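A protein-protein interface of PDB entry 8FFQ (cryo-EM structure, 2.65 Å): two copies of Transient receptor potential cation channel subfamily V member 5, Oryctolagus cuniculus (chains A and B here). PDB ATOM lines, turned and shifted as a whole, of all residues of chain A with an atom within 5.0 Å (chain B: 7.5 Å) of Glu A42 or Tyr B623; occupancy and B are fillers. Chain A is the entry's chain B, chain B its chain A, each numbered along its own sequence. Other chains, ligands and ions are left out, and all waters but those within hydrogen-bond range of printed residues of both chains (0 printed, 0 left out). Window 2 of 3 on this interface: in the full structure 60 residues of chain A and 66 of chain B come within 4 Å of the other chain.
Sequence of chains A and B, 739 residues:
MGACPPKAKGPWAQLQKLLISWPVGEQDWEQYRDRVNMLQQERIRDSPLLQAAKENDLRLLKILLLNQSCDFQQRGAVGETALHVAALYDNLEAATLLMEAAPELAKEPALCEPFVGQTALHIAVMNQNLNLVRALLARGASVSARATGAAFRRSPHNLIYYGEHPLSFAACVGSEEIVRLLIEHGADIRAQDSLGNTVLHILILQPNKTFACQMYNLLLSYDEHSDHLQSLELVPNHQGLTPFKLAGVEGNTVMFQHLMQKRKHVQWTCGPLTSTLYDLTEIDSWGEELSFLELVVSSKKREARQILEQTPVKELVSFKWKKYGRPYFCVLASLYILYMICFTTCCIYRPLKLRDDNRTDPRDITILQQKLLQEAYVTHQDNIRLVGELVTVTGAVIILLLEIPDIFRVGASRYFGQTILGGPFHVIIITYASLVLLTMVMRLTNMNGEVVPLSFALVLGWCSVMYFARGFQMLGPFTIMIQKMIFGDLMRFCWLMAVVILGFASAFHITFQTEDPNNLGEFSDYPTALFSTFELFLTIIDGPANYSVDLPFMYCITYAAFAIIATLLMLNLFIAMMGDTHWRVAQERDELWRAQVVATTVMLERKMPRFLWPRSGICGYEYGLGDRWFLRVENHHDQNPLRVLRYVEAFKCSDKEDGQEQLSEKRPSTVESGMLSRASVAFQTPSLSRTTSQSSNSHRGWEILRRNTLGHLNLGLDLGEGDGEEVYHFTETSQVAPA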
ATOM      1  N   ARG A  35      19.577 -13.321  -3.436  1.00  0.00           N
ATOM      2  CA  ARG A  35      18.470 -14.131  -2.913  1.00  0.00           C
ATOM      3  C   ARG A  35      18.394 -14.094  -1.392  1.00  0.00           C
ATOM      4  O   ARG A  35      17.320 -13.874  -0.855  1.00  0.00           O
ATOM      5  CB  ARG A  35      18.551 -15.570  -3.444  1.00  0.00           C
ATOM      6  CG  ARG A  35      17.434 -16.436  -2.853  1.00  0.00           C
ATOM      7  CD  ARG A  35      17.364 -17.827  -3.475  1.00  0.00           C
ATOM      8  NE  ARG A  35      16.197 -18.563  -2.956  1.00  0.00           N
ATOM      9  CZ  ARG A  35      14.968 -18.525  -3.430  1.00  0.00           C
ATOM     10  NH1 ARG A  35      14.021 -19.193  -2.857  1.00  0.00           N
ATOM     11  NH2 ARG A  35      14.653 -17.830  -4.476  1.00  0.00           N
ATOM     12  N   MET A  38      16.941 -10.758  -0.362  1.00  0.00           N
ATOM     13  CA  MET A  38      15.501 -10.747  -0.626  1.00  0.00           C
ATOM     14  C   MET A  38      14.726 -11.583   0.383  1.00  0.00           C
ATOM     15  O   MET A  38      13.679 -11.173   0.872  1.00  0.00           O
ATOM     16  CB  MET A  38      15.203 -11.294  -2.016  1.00  0.00           C
ATOM     17  CG  MET A  38      15.843 -10.531  -3.162  1.00  0.00           C
ATOM     18  SD  MET A  38      15.661  -8.745  -3.130  1.00  0.00           S
ATOM     19  CE  MET A  38      13.883  -8.636  -3.344  1.00  0.00           C
ATOM     20  N   LEU A  39      15.256 -12.749   0.726  1.00  0.00           N
ATOM     21  CA  LEU A  39      14.657 -13.721   1.622  1.00  0.00           C
ATOM     22  C   LEU A  39      14.661 -13.241   3.082  1.00  0.00           C
ATOM     23  O   LEU A  39      13.701 -13.479   3.809  1.00  0.00           O
ATOM     24  CB  LEU A  39      15.408 -15.041   1.390  1.00  0.00           C
ATOM     25  CG  LEU A  39      14.721 -16.311   1.893  1.00  0.00           C
ATOM     26  CD1 LEU A  39      13.403 -16.579   1.199  1.00  0.00           C
ATOM     27  CD2 LEU A  39      15.643 -17.485   1.635  1.00  0.00           C
ATOM     28  N   GLN A  40      15.682 -12.492   3.509  1.00  0.00           N
ATOM     29  CA  GLN A  40      15.693 -11.806   4.804  1.00  0.00           C
ATOM     30  C   GLN A  40      14.536 -10.819   4.911  1.00  0.00           C
ATOM     31  O   GLN A  40      13.761 -10.881   5.859  1.00  0.00           O
ATOM     32  CB  GLN A  40      17.028 -11.079   5.024  1.00  0.00           C
ATOM     33  CG  GLN A  40      18.149 -12.019   5.472  1.00  0.00           C
ATOM     34  CD  GLN A  40      19.500 -11.317   5.452  1.00  0.00           C
ATOM     35  OE1 GLN A  40      20.075 -11.052   4.414  1.00  0.00           O
ATOM     36  NE2 GLN A  40      20.052 -10.967   6.581  1.00  0.00           N
ATOM     37  N   GLN A  41      14.378  -9.947   3.921  1.00  0.00           N
ATOM     38  CA  GLN A  41      13.304  -8.958   3.896  1.00  0.00           C
ATOM     39  C   GLN A  41      11.920  -9.611   3.808  1.00  0.00           C
ATOM     40  O   GLN A  41      11.017  -9.191   4.515  1.00  0.00           O
ATOM     41  CB  GLN A  41      13.521  -7.988   2.732  1.00  0.00           C
ATOM     42  CG  GLN A  41      14.837  -7.211   2.818  1.00  0.00           C
ATOM     43  CD  GLN A  41      14.914  -6.253   3.990  1.00  0.00           C
ATOM     44  OE1 GLN A  41      13.987  -5.530   4.306  1.00  0.00           O
ATOM     45  NE2 GLN A  41      16.027  -6.198   4.674  1.00  0.00           N
ATOM     46  N   GLU A  42      11.769 -10.677   3.024  1.00  0.00           N
ATOM     47  CA  GLU A  42      10.562 -11.502   2.971  1.00  0.00           C
ATOM     48  C   GLU A  42      10.154 -11.997   4.365  1.00  0.00           C
ATOM     49  O   GLU A  42       9.031 -11.775   4.797  1.00  0.00           O
ATOM     50  CB  GLU A  42      10.836 -12.654   1.990  1.00  0.00           C
ATOM     51  CG  GLU A  42       9.842 -13.820   1.937  1.00  0.00           C
ATOM     52  CD  GLU A  42       8.502 -13.465   1.284  1.00  0.00           C
ATOM     53  OE1 GLU A  42       8.036 -12.322   1.446  1.00  0.00           O
ATOM     54  OE2 GLU A  42       7.919 -14.340   0.606  1.00  0.00           O
ATOM     55  N   ARG A  43      11.094 -12.470   5.153  1.00  0.00           N
ATOM     56  CA  ARG A  43      10.693 -13.042   6.455  1.00  0.00           C
ATOM     57  C   ARG A  43      10.327 -11.891   7.389  1.00  0.00           C
ATOM     58  O   ARG A  43       9.298 -11.992   8.088  1.00  0.00           O
ATOM     59  CB  ARG A  43      11.784 -13.970   6.980  1.00  0.00           C
ATOM     60  CG  ARG A  43      12.170 -15.074   6.014  1.00  0.00           C
ATOM     61  CD  ARG A  43      11.086 -16.120   5.937  1.00  0.00           C
ATOM     62  NE  ARG A  43      11.723 -17.417   5.814  1.00  0.00           N
ATOM     63  CZ  ARG A  43      12.247 -18.083   6.832  1.00  0.00           C
ATOM     64  NH1 ARG A  43      12.811 -19.260   6.627  1.00  0.00           N
ATOM     65  NH2 ARG A  43      12.213 -17.572   8.048  1.00  0.00           N
ATOM     66  N   ILE A  44      11.109 -10.836   7.371  1.00  0.00           N
ATOM     67  CA  ILE A  44      10.818  -9.660   8.193  1.00  0.00           C
ATOM     68  C   ILE A  44       9.404  -9.168   7.901  1.00  0.00           C
ATOM     69  O   ILE A  44       8.618  -9.003   8.823  1.00  0.00           O
ATOM     70  CB  ILE A  44      11.871  -8.556   7.985  1.00  0.00           C
ATOM     71  CG1 ILE A  44      13.247  -8.990   8.540  1.00  0.00           C
ATOM     72  CG2 ILE A  44      11.442  -7.239   8.654  1.00  0.00           C
ATOM     73  CD1 ILE A  44      14.412  -8.123   8.053  1.00  0.00           C
ATOM     74  N   ARG A  45       9.055  -8.994   6.627  1.00  0.00           N
ATOM     75  CA  ARG A  45       7.751  -8.515   6.167  1.00  0.00           C
ATOM     76  C   ARG A  45       6.625  -9.504   6.486  1.00  0.00           C
ATOM     77  O   ARG A  45       5.524  -9.090   6.827  1.00  0.00           O
ATOM     78  CB  ARG A  45       7.917  -8.210   4.673  1.00  0.00           C
ATOM     79  CG  ARG A  45       6.694  -7.618   3.988  1.00  0.00           C
ATOM     80  CD  ARG A  45       7.036  -6.944   2.655  1.00  0.00           C
ATOM     81  NE  ARG A  45       7.765  -7.829   1.725  1.00  0.00           N
ATOM     82  CZ  ARG A  45       8.997  -7.695   1.281  1.00  0.00           C
ATOM     83  NH1 ARG A  45       9.502  -8.556   0.458  1.00  0.00           N
ATOM     84  NH2 ARG A  45       9.760  -6.707   1.630  1.00  0.00           N
ATOM     85  N   ASP A  46       6.903 -10.803   6.451  1.00  0.00           N
ATOM     86  CA  ASP A  46       5.991 -11.877   6.865  1.00  0.00           C
ATOM     87  C   ASP A  46       5.715 -11.937   8.375  1.00  0.00           C
ATOM     88  O   ASP A  46       4.699 -12.505   8.778  1.00  0.00           O
ATOM     89  CB  ASP A  46       6.575 -13.241   6.453  1.00  0.00           C
ATOM     90  CG  ASP A  46       6.475 -13.578   4.965  1.00  0.00           C
ATOM     91  OD1 ASP A  46       5.699 -12.921   4.240  1.00  0.00           O
ATOM     92  OD2 ASP A  46       7.074 -14.594   4.552  1.00  0.00           O
ATOM     93  N   GLN B 267      16.937  -0.941   1.184  1.00  0.00           N
ATOM     94  CA  GLN B 267      16.567  -2.200   1.809  1.00  0.00           C
ATOM     95  C   GLN B 267      17.110  -2.320   3.239  1.00  0.00           C
ATOM     96  O   GLN B 267      16.375  -2.668   4.156  1.00  0.00           O
ATOM     97  CB  GLN B 267      17.133  -3.273   0.873  1.00  0.00           C
ATOM     98  CG  GLN B 267      16.483  -4.639   0.918  1.00  0.00           C
ATOM     99  CD  GLN B 267      17.052  -5.529  -0.177  1.00  0.00           C
ATOM    100  OE1 GLN B 267      18.166  -5.342  -0.635  1.00  0.00           O
ATOM    101  NE2 GLN B 267      16.332  -6.522  -0.632  1.00  0.00           N
ATOM    102  N   ILE B 618      15.998  -9.705 -10.410  1.00  0.00           N
ATOM    103  CA  ILE B 618      15.362 -10.481  -9.353  1.00  0.00           C
ATOM    104  C   ILE B 618      13.855 -10.436  -9.568  1.00  0.00           C
ATOM    105  O   ILE B 618      13.276  -9.352  -9.584  1.00  0.00           O
ATOM    106  CB  ILE B 618      15.745  -9.837  -8.003  1.00  0.00           C
ATOM    107  CG1 ILE B 618      17.268  -9.872  -7.748  1.00  0.00           C
ATOM    108  CG2 ILE B 618      15.013 -10.486  -6.829  1.00  0.00           C
ATOM    109  CD1 ILE B 618      17.725  -8.924  -6.643  1.00  0.00           C
ATOM    110  N   CYS B 619      13.198 -11.583  -9.695  1.00  0.00           N
ATOM    111  CA  CYS B 619      11.748 -11.631  -9.828  1.00  0.00           C
ATOM    112  C   CYS B 619      11.081 -11.279  -8.499  1.00  0.00           C
ATOM    113  O   CYS B 619      11.216 -12.008  -7.521  1.00  0.00           O
ATOM    114  CB  CYS B 619      11.337 -13.021 -10.310  1.00  0.00           C
ATOM    115  SG  CYS B 619       9.563 -13.025 -10.665  1.00  0.00           S
ATOM    116  N   GLY B 620      10.329 -10.180  -8.444  1.00  0.00           N
ATOM    117  CA  GLY B 620       9.649  -9.749  -7.227  1.00  0.00           C
ATOM    118  C   GLY B 620       8.596 -10.730  -6.715  1.00  0.00           C
ATOM    119  O   GLY B 620       8.363 -10.801  -5.510  1.00  0.00           O
ATOM    120  N   TYR B 621       7.988 -11.516  -7.603  1.00  0.00           N
ATOM    121  CA  TYR B 621       6.869 -12.396  -7.283  1.00  0.00           C
ATOM    122  C   TYR B 621       7.241 -13.489  -6.273  1.00  0.00           C
ATOM    123  O   TYR B 621       6.433 -13.815  -5.408  1.00  0.00           O
ATOM    124  CB  TYR B 621       6.326 -12.997  -8.584  1.00  0.00           C
ATOM    125  CG  TYR B 621       5.248 -14.040  -8.379  1.00  0.00           C
ATOM    126  CD1 TYR B 621       3.934 -13.653  -8.067  1.00  0.00           C
ATOM    127  CD2 TYR B 621       5.579 -15.404  -8.454  1.00  0.00           C
ATOM    128  CE1 TYR B 621       2.949 -14.628  -7.825  1.00  0.00           C
ATOM    129  CE2 TYR B 621       4.599 -16.382  -8.207  1.00  0.00           C
ATOM    130  CZ  TYR B 621       3.283 -15.995  -7.888  1.00  0.00           C
ATOM    131  OH  TYR B 621       2.340 -16.937  -7.633  1.00  0.00           O
ATOM    132  N   GLU B 622       8.475 -14.004  -6.301  1.00  0.00           N
ATOM    133  CA  GLU B 622       8.968 -14.965  -5.295  1.00  0.00           C
ATOM    134  C   GLU B 622       8.967 -14.420  -3.859  1.00  0.00           C
ATOM    135  O   GLU B 622       8.871 -15.233  -2.919  1.00  0.00           O
ATOM    136  CB  GLU B 622      10.391 -15.433  -5.648  1.00  0.00           C
ATOM    137  CG  GLU B 622      10.431 -16.284  -6.903  1.00  0.00           C
ATOM    138  CD  GLU B 622      11.765 -17.064  -7.010  1.00  0.00           C
ATOM    139  OE1 GLU B 622      12.321 -17.528  -5.960  1.00  0.00           O
ATOM    140  OE2 GLU B 622      12.267 -17.221  -8.146  1.00  0.00           O
ATOM    141  N   TYR B 623       9.059 -13.100  -3.684  1.00  0.00           N
ATOM    142  CA  TYR B 623       9.248 -12.436  -2.397  1.00  0.00           C
ATOM    143  C   TYR B 623       8.062 -11.547  -1.996  1.00  0.00           C
ATOM    144  O   TYR B 623       8.171 -10.757  -1.061  1.00  0.00           O
ATOM    145  CB  TYR B 623      10.577 -11.670  -2.399  1.00  0.00           C
ATOM    146  CG  TYR B 623      11.750 -12.449  -2.961  1.00  0.00           C
ATOM    147  CD1 TYR B 623      12.392 -13.432  -2.191  1.00  0.00           C
ATOM    148  CD2 TYR B 623      12.157 -12.221  -4.285  1.00  0.00           C
ATOM    149  CE1 TYR B 623      13.444 -14.183  -2.746  1.00  0.00           C
ATOM    150  CE2 TYR B 623      13.197 -12.973  -4.846  1.00  0.00           C
ATOM    151  CZ  TYR B 623      13.847 -13.954  -4.077  1.00  0.00           C
ATOM    152  OH  TYR B 623      14.857 -14.671  -4.622  1.00  0.00           O
ATOM    153  N   GLY B 624       6.933 -11.624  -2.706  1.00  0.00           N
ATOM    154  CA  GLY B 624       5.742 -10.831  -2.432  1.00  0.00           C
ATOM    155  C   GLY B 624       5.819  -9.390  -2.866  1.00  0.00           C
ATOM    156  O   GLY B 624       5.050  -8.567  -2.346  1.00  0.00           O
ATOM    157  N   LEU B 625       6.724  -9.027  -3.775  1.00  0.00           N
ATOM    158  CA  LEU B 625       6.864  -7.662  -4.298  1.00  0.00           C
ATOM    159  C   LEU B 625       6.010  -7.399  -5.558  1.00  0.00           C
ATOM    160  O   LEU B 625       6.174  -6.380  -6.224  1.00  0.00           O
ATOM    161  CB  LEU B 625       8.354  -7.354  -4.513  1.00  0.00           C
ATOM    162  CG  LEU B 625       9.222  -7.396  -3.248  1.00  0.00           C
ATOM    163  CD1 LEU B 625      10.689  -7.230  -3.624  1.00  0.00           C
ATOM    164  CD2 LEU B 625       8.854  -6.276  -2.282  1.00  0.00           C
ATOM    165  N   GLY B 626       5.090  -8.299  -5.896  1.00  0.00           N
ATOM    166  CA  GLY B 626       4.251  -8.205  -7.091  1.00  0.00           C
ATOM    167  C   GLY B 626       4.975  -8.582  -8.386  1.00  0.00           C
ATOM    168  O   GLY B 626       5.990  -9.272  -8.380  1.00  0.00           O
ATOM    169  N   PHE B 630      13.663  -6.512 -10.159  1.00  0.00           N
ATOM    170  CA  PHE B 630      14.548  -5.597  -9.450  1.00  0.00           C
ATOM    171  C   PHE B 630      16.020  -5.870  -9.712  1.00  0.00           C
ATOM    172  O   PHE B 630      16.402  -6.992 -10.004  1.00  0.00           O
ATOM    173  CB  PHE B 630      14.269  -5.646  -7.951  1.00  0.00           C
ATOM    174  CG  PHE B 630      12.857  -5.310  -7.539  1.00  0.00           C
ATOM    175  CD1 PHE B 630      12.479  -3.971  -7.345  1.00  0.00           C
ATOM    176  CD2 PHE B 630      11.915  -6.333  -7.370  1.00  0.00           C
ATOM    177  CE1 PHE B 630      11.160  -3.659  -6.993  1.00  0.00           C
ATOM    178  CE2 PHE B 630      10.597  -6.017  -7.024  1.00  0.00           C
ATOM    179  CZ  PHE B 630      10.221  -4.683  -6.829  1.00  0.00           C
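Hydrophobic or aromatic side chains of chain A within 4 Å of the printed part of chain B: Met A38. Of the 11 printed residues of chain B, 5 touch a printed residue of chain A. Among the printed residues, 11 pairs touch across the chains.
Glu A42 touches two residues of chain B. Printed residues of chain B within 4 Å of Met A38: Gln B267, Ile B618, Tyr B623 and Leu B625. Of the printed residues of chain A, Leu B625 touches Met A38 (3.5 Å) and Arg A45 (3.6 Å). Of the printed residues of chain B, Gln A41 touches Gln B267 (3.6 Å). Ile A44 touches none of the printed residues of chain B. Cys B619 touches none of the printed residues of chain A. The nearest printed residue of chain B that does not touch Gln A41 is Tyr B623 (6.3 Å).
Ile B618 touches Met A38. Tyr B623 touches Met A38. Leu B625 touches Met A38. Gln B267 touches Gln A41 (O to NE2, 3.6 Å). Glu B622 touches Glu A42 (O to OE2, 3.8 Å). Leu B625 touches Arg A45.
No position is printed for both chains. Of the 11 pairs that touch across the chains among the printed residues, none has its exchanged pair printed and touching as well.
OH of Tyr B623 lies within hydrogen-bond range of NH2 of Arg A35 (3.2 Å). The side-chain carboxylate (OE1) of Glu B622 is in salt-bridge range of the guanidinium group (NH2) of Arg A35 (2.8 Å). OE1 of Glu A42 sits close to O of Tyr B623, at 3.0 Å. The backbone carbonyl oxygen (O) of Tyr B623 sits at hydrogen-bond distance from the guanidinium group (NH1) of Arg A45, 3.0 Å away. The side-chain sulfur (SD) of Met A38 sits at hydrogen-bond distance from the side-chain amide nitrogen (NE2) of Gln B267.
The backbone NH of Leu B625 lies within hydrogen-bond range of the backbone carbonyl oxygen of Gly B620 (3.0 Å). The backbone NH (N) of Ile B618 is in hydrogen-bond range of the backbone carbonyl oxygen (O) of Phe B630 (2.8 Å).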
